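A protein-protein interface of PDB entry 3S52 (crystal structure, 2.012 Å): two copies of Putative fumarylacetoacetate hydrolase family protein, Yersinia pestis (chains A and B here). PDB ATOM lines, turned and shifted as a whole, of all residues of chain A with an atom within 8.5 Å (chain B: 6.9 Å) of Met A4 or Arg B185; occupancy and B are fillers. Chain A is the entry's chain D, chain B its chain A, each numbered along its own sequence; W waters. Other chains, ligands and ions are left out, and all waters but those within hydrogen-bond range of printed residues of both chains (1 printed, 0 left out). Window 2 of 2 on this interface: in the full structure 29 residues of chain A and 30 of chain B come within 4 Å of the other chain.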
ATOM      1  N   MET A   4      23.741  14.457  -6.118  1.00  0.00           N
ATOM      2  CA  MET A   4      22.473  14.549  -5.388  1.00  0.00           C
ATOM      3  C   MET A   4      21.455  13.559  -5.941  1.00  0.00           C
ATOM      4  O   MET A   4      21.324  13.434  -7.159  1.00  0.00           O
ATOM      5  CB  MET A   4      21.902  15.967  -5.461  1.00  0.00           C
ATOM      6  CG  MET A   4      20.565  16.112  -4.752  1.00  0.00           C
ATOM      7  SD  MET A   4      20.650  15.610  -2.868  1.00  0.00           S
ATOM      8  CE  MET A   4      21.778  17.077  -2.258  1.00  0.00           C
ATOM      9  N   TYR A   5      20.753  12.844  -5.063  1.00  0.00           N
ATOM     10  CA  TYR A   5      19.820  11.815  -5.526  1.00  0.00           C
ATOM     11  C   TYR A   5      18.612  12.432  -6.221  1.00  0.00           C
ATOM     12  O   TYR A   5      18.032  13.406  -5.739  1.00  0.00           O
ATOM     13  CB  TYR A   5      19.350  10.890  -4.390  1.00  0.00           C
ATOM     14  CG  TYR A   5      18.194  10.013  -4.827  1.00  0.00           C
ATOM     15  CD1 TYR A   5      18.414   8.781  -5.450  1.00  0.00           C
ATOM     16  CD2 TYR A   5      16.889  10.438  -4.672  1.00  0.00           C
ATOM     17  CE1 TYR A   5      17.346   7.984  -5.880  1.00  0.00           C
ATOM     18  CE2 TYR A   5      15.821   9.652  -5.092  1.00  0.00           C
ATOM     19  CZ  TYR A   5      16.058   8.430  -5.700  1.00  0.00           C
ATOM     20  OH  TYR A   5      14.999   7.670  -6.122  1.00  0.00           O
ATOM     21  N   GLN A   6      18.257  11.855  -7.361  1.00  0.00           N
ATOM     22  CA  GLN A   6      17.017  12.158  -8.060  1.00  0.00           C
ATOM     23  C   GLN A   6      16.421  10.833  -8.494  1.00  0.00           C
ATOM     24  O   GLN A   6      17.156   9.882  -8.749  1.00  0.00           O
ATOM     25  CB  GLN A   6      17.289  13.023  -9.292  1.00  0.00           C
ATOM     26  CG  GLN A   6      18.012  14.330  -8.978  1.00  0.00           C
ATOM     27  CD  GLN A   6      18.161  15.234 -10.193  1.00  0.00           C
ATOM     28  OE1 GLN A   6      19.241  15.332 -10.774  1.00  0.00           O
ATOM     29  NE2 GLN A   6      17.074  15.911 -10.572  1.00  0.00           N
ATOM     30  N   HIS A   7      15.096  10.770  -8.565  1.00  0.00           N
ATOM     31  CA  HIS A   7      14.404   9.589  -9.067  1.00  0.00           C
ATOM     32  C   HIS A   7      14.738   9.342 -10.534  1.00  0.00           C
ATOM     33  O   HIS A   7      14.784  10.279 -11.325  1.00  0.00           O
ATOM     34  CB  HIS A   7      12.892   9.773  -8.977  1.00  0.00           C
ATOM     35  CG  HIS A   7      12.376   9.952  -7.588  1.00  0.00           C
ATOM     36  ND1 HIS A   7      12.688   9.090  -6.559  1.00  0.00           N
ATOM     37  CD2 HIS A   7      11.539  10.878  -7.066  1.00  0.00           C
ATOM     38  CE1 HIS A   7      12.070   9.482  -5.459  1.00  0.00           C
ATOM     39  NE2 HIS A   7      11.363  10.564  -5.741  1.00  0.00           N
ATOM     40  N   ARG A   8      14.918   8.079 -10.901  1.00  0.00           N
ATOM     41  CA  ARG A   8      15.206   7.712 -12.288  1.00  0.00           C
ATOM     42  C   ARG A   8      14.406   6.489 -12.691  1.00  0.00           C
ATOM     43  O   ARG A   8      13.884   5.772 -11.835  1.00  0.00           O
ATOM     44  CB  ARG A   8      16.692   7.406 -12.444  1.00  0.00           C
ATOM     45  CG  ARG A   8      17.578   8.603 -12.185  1.00  0.00           C
ATOM     46  CD  ARG A   8      19.042   8.236 -12.124  1.00  0.00           C
ATOM     47  NE  ARG A   8      19.853   9.404 -11.768  1.00  0.00           N
ATOM     48  CZ  ARG A   8      20.206  10.352 -12.627  1.00  0.00           C
ATOM     49  NH1 ARG A   8      19.829  10.273 -13.896  1.00  0.00           N
ATOM     50  NH2 ARG A   8      20.940  11.379 -12.221  1.00  0.00           N
ATOM     51  N   LEU A  14      15.811  10.720 -15.930  1.00  0.00           N
ATOM     52  CA  LEU A  14      15.106  11.461 -14.882  1.00  0.00           C
ATOM     53  C   LEU A  14      13.580  11.364 -14.968  1.00  0.00           C
ATOM     54  O   LEU A  14      12.976  11.657 -16.006  1.00  0.00           O
ATOM     55  CB  LEU A  14      15.522  12.938 -14.897  1.00  0.00           C
ATOM     56  CG  LEU A  14      16.584  13.401 -13.890  1.00  0.00           C
ATOM     57  CD1 LEU A  14      17.833  12.545 -13.946  1.00  0.00           C
ATOM     58  CD2 LEU A  14      16.942  14.865 -14.114  1.00  0.00           C
ATOM     59  N   VAL A  19      11.669  14.587  -4.640  1.00  0.00           N
ATOM     60  CA  VAL A  19      12.114  13.635  -3.639  1.00  0.00           C
ATOM     61  C   VAL A  19      11.737  14.164  -2.265  1.00  0.00           C
ATOM     62  O   VAL A  19      11.918  15.355  -1.976  1.00  0.00           O
ATOM     63  CB  VAL A  19      13.621  13.429  -3.712  1.00  0.00           C
ATOM     64  CG1 VAL A  19      14.086  12.519  -2.586  1.00  0.00           C
ATOM     65  CG2 VAL A  19      13.992  12.845  -5.079  1.00  0.00           C
ATOM     66  N   PRO A  50      14.505   9.745   5.872  1.00  0.00           N
ATOM     67  CA  PRO A  50      14.358  11.042   5.209  1.00  0.00           C
ATOM     68  C   PRO A  50      15.080  11.058   3.865  1.00  0.00           C
ATOM     69  O   PRO A  50      15.796  10.111   3.511  1.00  0.00           O
ATOM     70  CB  PRO A  50      15.070  11.993   6.180  1.00  0.00           C
ATOM     71  CG  PRO A  50      16.202  11.140   6.720  1.00  0.00           C
ATOM     72  CD  PRO A  50      15.592   9.747   6.866  1.00  0.00           C
ATOM     73  N   GLU A  51      14.921  12.159   3.143  1.00  0.00           N
ATOM     74  CA  GLU A  51      15.522  12.319   1.832  1.00  0.00           C
ATOM     75  C   GLU A  51      17.048  12.123   1.860  1.00  0.00           C
ATOM     76  O   GLU A  51      17.634  11.663   0.883  1.00  0.00           O
ATOM     77  CB  GLU A  51      15.157  13.706   1.276  1.00  0.00           C
ATOM     78  CG  GLU A  51      16.057  14.211   0.157  1.00  0.00           C
ATOM     79  CD  GLU A  51      17.316  14.899   0.673  1.00  0.00           C
ATOM     80  OE1 GLU A  51      17.225  15.682   1.645  1.00  0.00           O
ATOM     81  OE2 GLU A  51      18.399  14.648   0.103  1.00  0.00           O
ATOM     82  N   THR A  52      17.690  12.456   2.975  1.00  0.00           N
ATOM     83  CA  THR A  52      19.151  12.331   3.054  1.00  0.00           C
ATOM     84  C   THR A  52      19.626  10.874   3.145  1.00  0.00           C
ATOM     85  O   THR A  52      20.823  10.598   3.032  1.00  0.00           O
ATOM     86  CB  THR A  52      19.722  13.141   4.240  1.00  0.00           C
ATOM     87  OG1 THR A  52      18.880  12.950   5.380  1.00  0.00           O
ATOM     88  CG2 THR A  52      19.758  14.633   3.900  1.00  0.00           C
ATOM     89  N   ALA A  53      18.693   9.946   3.363  1.00  0.00           N
ATOM     90  CA  ALA A  53      19.021   8.515   3.343  1.00  0.00           C
ATOM     91  C   ALA A  53      19.233   7.984   1.921  1.00  0.00           C
ATOM     92  O   ALA A  53      19.936   6.991   1.709  1.00  0.00           O
ATOM     93  CB  ALA A  53      17.905   7.690   4.048  1.00  0.00           C
ATOM     94  N   LEU A  54      18.613   8.642   0.950  1.00  0.00           N
ATOM     95  CA  LEU A  54      18.537   8.116  -0.414  1.00  0.00           C
ATOM     96  C   LEU A  54      19.821   8.307  -1.202  1.00  0.00           C
ATOM     97  O   LEU A  54      20.468   9.344  -1.111  1.00  0.00           O
ATOM     98  CB  LEU A  54      17.402   8.804  -1.171  1.00  0.00           C
ATOM     99  CG  LEU A  54      16.004   8.396  -0.731  1.00  0.00           C
ATOM    100  CD1 LEU A  54      14.988   9.385  -1.240  1.00  0.00           C
ATOM    101  CD2 LEU A  54      15.727   6.999  -1.278  1.00  0.00           C
ATOM    102  N   CYS A  55      20.183   7.309  -1.994  1.00  0.00           N
ATOM    103  CA  CYS A  55      21.318   7.453  -2.888  1.00  0.00           C
ATOM    104  C   CYS A  55      21.196   6.459  -4.038  1.00  0.00           C
ATOM    105  O   CYS A  55      20.433   5.480  -3.976  1.00  0.00           O
ATOM    106  CB  CYS A  55      22.646   7.291  -2.140  1.00  0.00           C
ATOM    107  SG  CYS A  55      22.845   5.663  -1.350  1.00  0.00           S
ATOM    108  N   ASP A  56      21.951   6.709  -5.094  1.00  0.00           N
ATOM    109  CA  ASP A  56      21.848   5.889  -6.297  1.00  0.00           C
ATOM    110  C   ASP A  56      22.609   4.568  -6.091  1.00  0.00           C
ATOM    111  O   ASP A  56      23.818   4.558  -5.897  1.00  0.00           O
ATOM    112  CB  ASP A  56      22.383   6.708  -7.480  1.00  0.00           C
ATOM    113  CG  ASP A  56      22.601   5.889  -8.726  1.00  0.00           C
ATOM    114  OD1 ASP A  56      22.188   4.710  -8.753  1.00  0.00           O
ATOM    115  OD2 ASP A  56      23.184   6.445  -9.692  1.00  0.00           O
ATOM    116  N   ASP A 128      22.498   8.862   7.045  1.00  0.00           N
ATOM    117  CA  ASP A 128      22.821   9.282   5.693  1.00  0.00           C
ATOM    118  C   ASP A 128      23.191   8.075   4.853  1.00  0.00           C
ATOM    119  O   ASP A 128      24.002   7.272   5.283  1.00  0.00           O
ATOM    120  CB  ASP A 128      24.035  10.211   5.714  1.00  0.00           C
ATOM    121  CG  ASP A 128      23.673  11.660   5.930  1.00  0.00           C
ATOM    122  OD1 ASP A 128      22.503  11.988   6.265  1.00  0.00           O
ATOM    123  OD2 ASP A 128      24.596  12.474   5.772  1.00  0.00           O
ATOM    124  N   GLY A 129      22.608   7.966   3.661  1.00  0.00           N
ATOM    125  CA  GLY A 129      22.961   6.917   2.714  1.00  0.00           C
ATOM    126  C   GLY A 129      22.368   5.558   3.058  1.00  0.00           C
ATOM    127  O   GLY A 129      22.801   4.542   2.519  1.00  0.00           O
ATOM    128  N   PRO B  18      14.640  25.677   1.856  1.00  0.00           N
ATOM    129  CA  PRO B  18      13.883  24.443   1.594  1.00  0.00           C
ATOM    130  C   PRO B  18      13.280  23.818   2.867  1.00  0.00           C
ATOM    131  O   PRO B  18      13.736  24.047   3.983  1.00  0.00           O
ATOM    132  CB  PRO B  18      14.953  23.494   1.030  1.00  0.00           C
ATOM    133  CG  PRO B  18      16.068  24.372   0.588  1.00  0.00           C
ATOM    134  CD  PRO B  18      16.071  25.524   1.535  1.00  0.00           C
ATOM    135  N   ASN B  20      12.539  20.137   4.518  1.00  0.00           N
ATOM    136  CA  ASN B  20      12.738  18.689   4.387  1.00  0.00           C
ATOM    137  C   ASN B  20      12.345  17.907   5.621  1.00  0.00           C
ATOM    138  O   ASN B  20      11.391  17.123   5.594  1.00  0.00           O
ATOM    139  CB  ASN B  20      14.187  18.356   3.998  1.00  0.00           C
ATOM    140  CG  ASN B  20      14.486  18.695   2.557  1.00  0.00           C
ATOM    141  OD1 ASN B  20      15.088  19.741   2.254  1.00  0.00           O
ATOM    142  ND2 ASN B  20      14.055  17.821   1.648  1.00  0.00           N
ATOM    143  N   LYS B  21      13.092  18.100   6.705  1.00  0.00           N
ATOM    144  CA  LYS B  21      12.862  17.306   7.911  1.00  0.00           C
ATOM    145  C   LYS B  21      13.053  18.105   9.191  1.00  0.00           C
ATOM    146  O   LYS B  21      13.565  19.233   9.180  1.00  0.00           O
ATOM    147  CB  LYS B  21      13.762  16.055   7.941  1.00  0.00           C
ATOM    148  CG  LYS B  21      15.279  16.360   8.048  1.00  0.00           C
ATOM    149  CD  LYS B  21      16.111  15.065   8.108  1.00  0.00           C
ATOM    150  CE  LYS B  21      17.626  15.351   7.995  1.00  0.00           C
ATOM    151  NZ  LYS B  21      17.998  16.019   6.698  1.00  0.00           N
ATOM    152  N   LEU B  79      16.366  26.796  13.402  1.00  0.00           N
ATOM    153  CA  LEU B  79      16.404  26.710  11.945  1.00  0.00           C
ATOM    154  C   LEU B  79      17.849  26.682  11.468  1.00  0.00           C
ATOM    155  O   LEU B  79      18.645  27.569  11.802  1.00  0.00           O
ATOM    156  CB  LEU B  79      15.665  27.910  11.328  1.00  0.00           C
ATOM    157  CG  LEU B  79      15.578  28.041   9.796  1.00  0.00           C
ATOM    158  CD1 LEU B  79      14.872  26.865   9.157  1.00  0.00           C
ATOM    159  CD2 LEU B  79      14.885  29.341   9.402  1.00  0.00           C
ATOM    160  N   ILE B  80      18.186  25.663  10.684  1.00  0.00           N
ATOM    161  CA  ILE B  80      19.517  25.547  10.125  1.00  0.00           C
ATOM    162  C   ILE B  80      19.590  26.327   8.805  1.00  0.00           C
ATOM    163  O   ILE B  80      18.753  26.138   7.926  1.00  0.00           O
ATOM    164  CB  ILE B  80      19.910  24.072   9.867  1.00  0.00           C
ATOM    165  CG1 ILE B  80      19.715  23.208  11.126  1.00  0.00           C
ATOM    166  CG2 ILE B  80      21.343  23.995   9.355  1.00  0.00           C
ATOM    167  CD1 ILE B  80      20.494  23.693  12.336  1.00  0.00           C
ATOM    168  N   GLY B  81      20.577  27.211   8.674  1.00  0.00           N
ATOM    169  CA  GLY B  81      20.733  27.999   7.455  1.00  0.00           C
ATOM    170  C   GLY B  81      21.875  27.567   6.549  1.00  0.00           C
ATOM    171  O   GLY B  81      21.997  28.054   5.423  1.00  0.00           O
ATOM    172  N   THR B  82      22.721  26.665   7.043  1.00  0.00           N
ATOM    173  CA  THR B  82      23.878  26.182   6.293  1.00  0.00           C
ATOM    174  C   THR B  82      24.005  24.694   6.545  1.00  0.00           C
ATOM    175  O   THR B  82      23.915  24.269   7.686  1.00  0.00           O
ATOM    176  CB  THR B  82      25.173  26.855   6.808  1.00  0.00           C
ATOM    177  OG1 THR B  82      25.039  28.282   6.755  1.00  0.00           O
ATOM    178  CG2 THR B  82      26.386  26.420   5.991  1.00  0.00           C
ATOM    179  N   PRO B  83      24.289  23.900   5.500  1.00  0.00           N
ATOM    180  CA  PRO B  83      24.250  22.451   5.723  1.00  0.00           C
ATOM    181  C   PRO B  83      25.316  21.984   6.701  1.00  0.00           C
ATOM    182  O   PRO B  83      26.433  22.511   6.751  1.00  0.00           O
ATOM    183  CB  PRO B  83      24.478  21.863   4.323  1.00  0.00           C
ATOM    184  CG  PRO B  83      25.159  22.966   3.544  1.00  0.00           C
ATOM    185  CD  PRO B  83      24.594  24.248   4.101  1.00  0.00           C
ATOM    186  N   LEU B  84      24.956  20.999   7.510  1.00  0.00           N
ATOM    187  CA  LEU B  84      25.880  20.465   8.506  1.00  0.00           C
ATOM    188  C   LEU B  84      25.987  18.951   8.392  1.00  0.00           C
ATOM    189  O   LEU B  84      24.967  18.247   8.394  1.00  0.00           O
ATOM    190  CB  LEU B  84      25.402  20.828   9.903  1.00  0.00           C
ATOM    191  CG  LEU B  84      25.337  22.313  10.219  1.00  0.00           C
ATOM    192  CD1 LEU B  84      24.429  22.558  11.432  1.00  0.00           C
ATOM    193  CD2 LEU B  84      26.752  22.873  10.442  1.00  0.00           C
ATOM    194  N   PHE B 182      22.748  12.372  10.729  1.00  0.00           N
ATOM    195  CA  PHE B 182      21.950  12.965   9.659  1.00  0.00           C
ATOM    196  C   PHE B 182      22.557  14.260   9.118  1.00  0.00           C
ATOM    197  O   PHE B 182      22.905  15.161   9.875  1.00  0.00           O
ATOM    198  CB  PHE B 182      20.526  13.208  10.162  1.00  0.00           C
ATOM    199  CG  PHE B 182      20.026  12.119  11.078  1.00  0.00           C
ATOM    200  CD1 PHE B 182      19.765  10.849  10.585  1.00  0.00           C
ATOM    201  CD2 PHE B 182      19.828  12.359  12.422  1.00  0.00           C
ATOM    202  CE1 PHE B 182      19.312   9.843  11.419  1.00  0.00           C
ATOM    203  CE2 PHE B 182      19.373  11.352  13.258  1.00  0.00           C
ATOM    204  CZ  PHE B 182      19.129  10.095  12.752  1.00  0.00           C
ATOM    205  N   THR B 183      22.725  14.334   7.805  1.00  0.00           N
ATOM    206  CA  THR B 183      23.070  15.619   7.207  1.00  0.00           C
ATOM    207  C   THR B 183      21.898  16.558   7.478  1.00  0.00           C
ATOM    208  O   THR B 183      20.746  16.227   7.193  1.00  0.00           O
ATOM    209  CB  THR B 183      23.307  15.500   5.688  1.00  0.00           C
ATOM    210  OG1 THR B 183      24.562  14.847   5.457  1.00  0.00           O
ATOM    211  CG2 THR B 183      23.327  16.895   5.025  1.00  0.00           C
ATOM    212  N   LEU B 184      22.177  17.716   8.059  1.00  0.00           N
ATOM    213  CA  LEU B 184      21.132  18.701   8.294  1.00  0.00           C
ATOM    214  C   LEU B 184      21.215  19.764   7.208  1.00  0.00           C
ATOM    215  O   LEU B 184      22.148  20.564   7.190  1.00  0.00           O
ATOM    216  CB  LEU B 184      21.275  19.330   9.679  1.00  0.00           C
ATOM    217  CG  LEU B 184      21.383  18.367  10.864  1.00  0.00           C
ATOM    218  CD1 LEU B 184      21.402  19.132  12.173  1.00  0.00           C
ATOM    219  CD2 LEU B 184      20.252  17.350  10.851  1.00  0.00           C
ATOM    220  N   ARG B 185      20.255  19.756   6.290  1.00  0.00           N
ATOM    221  CA  ARG B 185      20.308  20.668   5.163  1.00  0.00           C
ATOM    222  C   ARG B 185      19.856  22.051   5.611  1.00  0.00           C
ATOM    223  O   ARG B 185      19.145  22.188   6.609  1.00  0.00           O
ATOM    224  CB  ARG B 185      19.434  20.153   4.022  1.00  0.00           C
ATOM    225  CG  ARG B 185      19.822  18.753   3.478  1.00  0.00           C
ATOM    226  CD  ARG B 185      19.363  18.582   2.018  1.00  0.00           C
ATOM    227  NE  ARG B 185      19.505  17.217   1.487  1.00  0.00           N
ATOM    228  CZ  ARG B 185      20.660  16.685   1.094  1.00  0.00           C
ATOM    229  NH1 ARG B 185      20.697  15.451   0.609  1.00  0.00           N
ATOM    230  NH2 ARG B 185      21.784  17.381   1.196  1.00  0.00           N
ATOM    231  N   ALA B 186      20.278  23.073   4.881  1.00  0.00           N
ATOM    232  CA  ALA B 186      19.707  24.396   5.069  1.00  0.00           C
ATOM    233  C   ALA B 186      18.198  24.232   4.988  1.00  0.00           C
ATOM    234  O   ALA B 186      17.694  23.560   4.090  1.00  0.00           O
ATOM    235  CB  ALA B 186      20.196  25.343   3.976  1.00  0.00           C
ATOM    236  N   GLY B 187      17.477  24.816   5.939  1.00  0.00           N
ATOM    237  CA  GLY B 187      16.033  24.689   5.964  1.00  0.00           C
ATOM    238  C   GLY B 187      15.556  23.568   6.872  1.00  0.00           C
ATOM    239  O   GLY B 187      14.362  23.452   7.130  1.00  0.00           O
ATOM    240  N   ASP B 188      16.468  22.724   7.355  1.00  0.00           N
ATOM    241  CA  ASP B 188      16.037  21.724   8.325  1.00  0.00           C
ATOM    242  C   ASP B 188      15.803  22.407   9.660  1.00  0.00           C
ATOM    243  O   ASP B 188      16.340  23.480   9.925  1.00  0.00           O
ATOM    244  CB  ASP B 188      17.018  20.561   8.468  1.00  0.00           C
ATOM    245  CG  ASP B 188      16.924  19.559   7.305  1.00  0.00           C
ATOM    246  OD1 ASP B 188      15.936  19.580   6.537  1.00  0.00           O
ATOM    247  OD2 ASP B 188      17.844  18.735   7.166  1.00  0.00           O
ATOM    248  N   ILE B 189      14.990  21.781  10.498  1.00  0.00           N
ATOM    249  CA  ILE B 189      14.653  22.341  11.789  1.00  0.00           C
ATOM    250  C   ILE B 189      15.104  21.352  12.852  1.00  0.00           C
ATOM    251  O   ILE B 189      15.001  20.136  12.660  1.00  0.00           O
ATOM    252  CB  ILE B 189      13.115  22.567  11.892  1.00  0.00           C
ATOM    253  CG1 ILE B 189      12.633  23.568  10.832  1.00  0.00           C
ATOM    254  CG2 ILE B 189      12.713  23.005  13.281  1.00  0.00           C
ATOM    255  CD1 ILE B 189      11.110  23.560  10.629  1.00  0.00           C
HETATM  256  O   HOH W   1      16.462  15.124   4.400  1.00  0.00           O
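The side-chain hydroxyl (OG1) of Thr A52 sits at hydrogen-bond distance from the side-chain amino group (NZ) of Lys B21.
The backbone NH of Thr B183 sits at hydrogen-bond distance from the side-chain carboxylate of Asp A128.
SD of Met A4 lies close to NH1 of Arg B185.
The guanidinium group (NH1) of Arg B185 lies within salt-bridge range of the side-chain carboxylate (OE2) of Glu A51 (2.5 Å).
The side-chain amino group (NZ) of Lys B21 lies within hydrogen-bond range of the backbone carbonyl oxygen (O) of Thr B183, 2.8 Å away.
The side-chain amino group (NZ) of Lys B21 lies within salt-bridge range of the side-chain carboxylate (OD2) of Asp B188 (2.8 Å).
The backbone carbonyl oxygen (O) of Lys B21 lies within hydrogen-bond range of the backbone NH (N) of Ile B189 (3.2 Å).
OD2 of Asp B188 is in hydrogen-bond range of N of Arg B185 (2.8 Å).
The backbone NH of Gly A129 is in hydrogen-bond range of the backbone carbonyl oxygen of Thr A52 (3.2 Å).
Lys B21 touches Pro A50.
Asn B20 touches Glu A51 (ND2 to OE1, 3.8 Å).
Thr A52 touches Thr B183 (CG2 to O, 3.8 Å).
Thr A52 touches Arg B185 (CG2 to NH1, 3.5 Å).
OD1 of Asp A128 touches CA of Phe B182 (3.6 Å).
Of the printed residues of chain B, Met A4 touches Arg B185 (3.5 Å).
Printed residues of chain A within 4 Å of Arg B185: Met A4, Glu A51 and Thr A52.
No residue of chain A comes within 4 Å of Ala B186.
Of the printed residues of chain B, Pro A50 touches Lys B21 (3.8 Å).
Of the printed residues of chain B, Glu A51 touches Asn B20 (3.8 Å) and Arg B185 (2.5 Å).
Of the printed residues of chain A, Asn B20 touches Glu A51 (3.8 Å).
The nearest residue of chain A that does not touch Arg B185 is Tyr A5 (6.2 Å).
Among the printed residues, Asp or Glu carboxylates within 4 Å of a Lys or Arg side-chain nitrogen of the other chain: Glu A51 with Arg B185.
No position is printed for both chains.
Of the 9 pairs that touch across the chains among the printed residues, none has its exchanged pair printed and touching as well.
Water W1 lies within hydrogen-bond range of NZ of Lys B21 (2.9 Å), OE1 of Glu A51 (2.9 Å) and N of Thr A52 (3.3 Å).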
